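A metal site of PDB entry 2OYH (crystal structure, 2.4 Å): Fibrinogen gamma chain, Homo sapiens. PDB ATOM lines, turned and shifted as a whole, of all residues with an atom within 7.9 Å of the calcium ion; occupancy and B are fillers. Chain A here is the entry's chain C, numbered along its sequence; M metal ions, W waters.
The backbone NH (N) of Cys 231 sits at hydrogen-bond distance from the side-chain carboxylate (OD2) of Asp 225 (3.0 Å).
The side-chain hydroxyl of Ser 218 lies within hydrogen-bond range of the backbone NH of Asp 225.
Of the 13 residues printed, 4 come within 4 Å of the calcium ion.
The nearest printed residue that does not touch the calcium ion is Glu 228 (4.01 Å).
The backbone carbonyl oxygen (O) of Phe 227 binds the calcium ion, 2.1 Å away.
The side-chain carboxylate (OD1) of Asp 225 binds the calcium ion, at 2.3 Å.
O of Gly 229 binds the calcium ion (2.4 Å).
The calcium ion is bound by water W1 (2.6 Å).
The calcium ion is bound by OD2 of Asp 223 (2.6 Å).
OD1 of Asp 223 is bound to the calcium ion, 2.7 Å away.
The calcium ion has six donor atoms within binding distance.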
ATOM      1  N   SER A 218     -10.214 -32.974  -9.591  1.00  0.00           N
ATOM      2  CA  SER A 218     -10.050 -32.817  -8.152  1.00  0.00           C
ATOM      3  C   SER A 218     -10.604 -33.969  -7.316  1.00  0.00           C
ATOM      4  O   SER A 218     -11.621 -34.579  -7.654  1.00  0.00           O
ATOM      5  CB  SER A 218     -10.713 -31.514  -7.675  1.00  0.00           C
ATOM      6  OG  SER A 218     -10.049 -30.372  -8.165  1.00  0.00           O
ATOM      7  N   ASN A 222      -6.540 -33.849  -3.129  1.00  0.00           N
ATOM      8  CA  ASN A 222      -5.856 -33.085  -4.155  1.00  0.00           C
ATOM      9  C   ASN A 222      -6.845 -32.080  -4.755  1.00  0.00           C
ATOM     10  O   ASN A 222      -7.504 -32.355  -5.761  1.00  0.00           O
ATOM     11  CB  ASN A 222      -5.286 -34.019  -5.235  1.00  0.00           C
ATOM     12  CG  ASN A 222      -4.288 -33.320  -6.143  1.00  0.00           C
ATOM     13  OD1 ASN A 222      -3.499 -33.968  -6.827  1.00  0.00           O
ATOM     14  ND2 ASN A 222      -4.322 -31.995  -6.149  1.00  0.00           N
ATOM     15  N   ASP A 223      -6.947 -30.925  -4.099  1.00  0.00           N
ATOM     16  CA  ASP A 223      -7.850 -29.841  -4.497  1.00  0.00           C
ATOM     17  C   ASP A 223      -7.277 -28.980  -5.629  1.00  0.00           C
ATOM     18  O   ASP A 223      -6.215 -28.368  -5.481  1.00  0.00           O
ATOM     19  CB  ASP A 223      -8.133 -28.933  -3.298  1.00  0.00           C
ATOM     20  CG  ASP A 223      -9.245 -27.917  -3.558  1.00  0.00           C
ATOM     21  OD1 ASP A 223      -9.305 -27.366  -4.677  1.00  0.00           O
ATOM     22  OD2 ASP A 223     -10.036 -27.666  -2.630  1.00  0.00           O
ATOM     23  N   ASN A 224      -7.991 -28.923  -6.754  1.00  0.00           N
ATOM     24  CA  ASN A 224      -7.566 -28.114  -7.901  1.00  0.00           C
ATOM     25  C   ASN A 224      -8.769 -27.369  -8.471  1.00  0.00           C
ATOM     26  O   ASN A 224      -8.817 -27.070  -9.664  1.00  0.00           O
ATOM     27  CB  ASN A 224      -6.947 -28.993  -8.993  1.00  0.00           C
ATOM     28  CG  ASN A 224      -5.763 -29.817  -8.491  1.00  0.00           C
ATOM     29  OD1 ASN A 224      -5.896 -31.003  -8.193  1.00  0.00           O
ATOM     30  ND2 ASN A 224      -4.598 -29.187  -8.386  1.00  0.00           N
ATOM     31  N   ASP A 225      -9.735 -27.073  -7.601  1.00  0.00           N
ATOM     32  CA  ASP A 225     -10.958 -26.380  -8.000  1.00  0.00           C
ATOM     33  C   ASP A 225     -10.888 -24.854  -7.807  1.00  0.00           C
ATOM     34  O   ASP A 225      -9.955 -24.336  -7.187  1.00  0.00           O
ATOM     35  CB  ASP A 225     -12.145 -26.920  -7.215  1.00  0.00           C
ATOM     36  CG  ASP A 225     -12.023 -26.650  -5.722  1.00  0.00           C
ATOM     37  OD1 ASP A 225     -11.584 -25.532  -5.355  1.00  0.00           O
ATOM     38  OD2 ASP A 225     -12.374 -27.536  -4.920  1.00  0.00           O
ATOM     39  N   LYS A 226     -11.888 -24.159  -8.341  1.00  0.00           N
ATOM     40  CA  LYS A 226     -11.977 -22.704  -8.233  1.00  0.00           C
ATOM     41  C   LYS A 226     -12.864 -22.334  -7.042  1.00  0.00           C
ATOM     42  O   LYS A 226     -13.813 -21.578  -7.197  1.00  0.00           O
ATOM     43  CB  LYS A 226     -12.581 -22.120  -9.513  1.00  0.00           C
ATOM     44  CG  LYS A 226     -11.872 -22.529 -10.806  1.00  0.00           C
ATOM     45  CD  LYS A 226     -10.375 -22.268 -10.732  1.00  0.00           C
ATOM     46  CE  LYS A 226      -9.686 -22.586 -12.043  1.00  0.00           C
ATOM     47  NZ  LYS A 226      -8.205 -22.595 -11.891  1.00  0.00           N
ATOM     48  N   PHE A 227     -12.540 -22.863  -5.876  1.00  0.00           N
ATOM     49  CA  PHE A 227     -13.322 -22.600  -4.676  1.00  0.00           C
ATOM     50  C   PHE A 227     -12.362 -22.583  -3.487  1.00  0.00           C
ATOM     51  O   PHE A 227     -11.441 -23.385  -3.418  1.00  0.00           O
ATOM     52  CB  PHE A 227     -14.378 -23.700  -4.516  1.00  0.00           C
ATOM     53  CG  PHE A 227     -15.248 -23.558  -3.297  1.00  0.00           C
ATOM     54  CD1 PHE A 227     -15.870 -22.359  -2.984  1.00  0.00           C
ATOM     55  CD2 PHE A 227     -15.494 -24.669  -2.487  1.00  0.00           C
ATOM     56  CE1 PHE A 227     -16.715 -22.253  -1.885  1.00  0.00           C
ATOM     57  CE2 PHE A 227     -16.343 -24.582  -1.377  1.00  0.00           C
ATOM     58  CZ  PHE A 227     -16.959 -23.378  -1.079  1.00  0.00           C
ATOM     59  N   GLU A 228     -12.567 -21.652  -2.563  1.00  0.00           N
ATOM     60  CA  GLU A 228     -11.699 -21.564  -1.408  1.00  0.00           C
ATOM     61  C   GLU A 228     -11.851 -22.824  -0.577  1.00  0.00           C
ATOM     62  O   GLU A 228     -10.952 -23.207   0.166  1.00  0.00           O
ATOM     63  CB  GLU A 228     -12.047 -20.335  -0.554  1.00  0.00           C
ATOM     64  CG  GLU A 228     -13.385 -20.428   0.156  1.00  0.00           C
ATOM     65  CD  GLU A 228     -13.615 -19.256   1.080  1.00  0.00           C
ATOM     66  OE1 GLU A 228     -14.614 -19.281   1.838  1.00  0.00           O
ATOM     67  OE2 GLU A 228     -12.797 -18.294   1.054  1.00  0.00           O
ATOM     68  N   GLY A 229     -12.997 -23.484  -0.724  1.00  0.00           N
ATOM     69  CA  GLY A 229     -13.238 -24.721  -0.015  1.00  0.00           C
ATOM     70  C   GLY A 229     -12.761 -25.901  -0.851  1.00  0.00           C
ATOM     71  O   GLY A 229     -11.979 -25.729  -1.782  1.00  0.00           O
ATOM     72  N   ASN A 230     -13.252 -27.084  -0.525  1.00  0.00           N
ATOM     73  CA  ASN A 230     -12.854 -28.284  -1.249  1.00  0.00           C
ATOM     74  C   ASN A 230     -14.066 -29.019  -1.812  1.00  0.00           C
ATOM     75  O   ASN A 230     -14.650 -29.864  -1.153  1.00  0.00           O
ATOM     76  CB  ASN A 230     -12.074 -29.206  -0.308  1.00  0.00           C
ATOM     77  CG  ASN A 230     -11.411 -30.368  -1.018  1.00  0.00           C
ATOM     78  OD1 ASN A 230     -10.458 -30.949  -0.512  1.00  0.00           O
ATOM     79  ND2 ASN A 230     -11.924 -30.720  -2.199  1.00  0.00           N
ATOM     80  N   CYS A 231     -14.430 -28.687  -3.056  1.00  0.00           N
ATOM     81  CA  CYS A 231     -15.587 -29.296  -3.698  1.00  0.00           C
ATOM     82  C   CYS A 231     -15.572 -30.813  -3.601  1.00  0.00           C
ATOM     83  O   CYS A 231     -16.505 -31.417  -3.067  1.00  0.00           O
ATOM     84  CB  CYS A 231     -15.658 -28.894  -5.182  1.00  0.00           C
ATOM     85  SG  CYS A 231     -15.979 -27.138  -5.556  1.00  0.00           S
ATOM     86  N   ALA A 232     -14.522 -31.425  -4.130  1.00  0.00           N
ATOM     87  CA  ALA A 232     -14.389 -32.881  -4.113  1.00  0.00           C
ATOM     88  C   ALA A 232     -14.654 -33.476  -2.733  1.00  0.00           C
ATOM     89  O   ALA A 232     -15.293 -34.523  -2.614  1.00  0.00           O
ATOM     90  CB  ALA A 232     -13.000 -33.275  -4.600  1.00  0.00           C
ATOM     91  N   ASN A 242     -15.285 -26.943 -10.431  1.00  0.00           N
ATOM     92  CA  ASN A 242     -15.141 -25.500 -10.636  1.00  0.00           C
ATOM     93  C   ASN A 242     -15.484 -24.870  -9.269  1.00  0.00           C
ATOM     94  O   ASN A 242     -14.615 -24.757  -8.408  1.00  0.00           O
ATOM     95  CB  ASN A 242     -16.122 -25.019 -11.709  1.00  0.00           C
ATOM     96  CG  ASN A 242     -15.883 -23.584 -12.127  1.00  0.00           C
ATOM     97  OD1 ASN A 242     -15.639 -22.709 -11.288  1.00  0.00           O
ATOM     98  ND2 ASN A 242     -15.966 -23.323 -13.434  1.00  0.00           N
HETATM   99 CA    CA M   1     -10.318 -25.181  -3.434  1.00  0.00          CA
HETATM  100  O   HOH W   1      -8.607 -24.342  -1.683  1.00  0.00           O
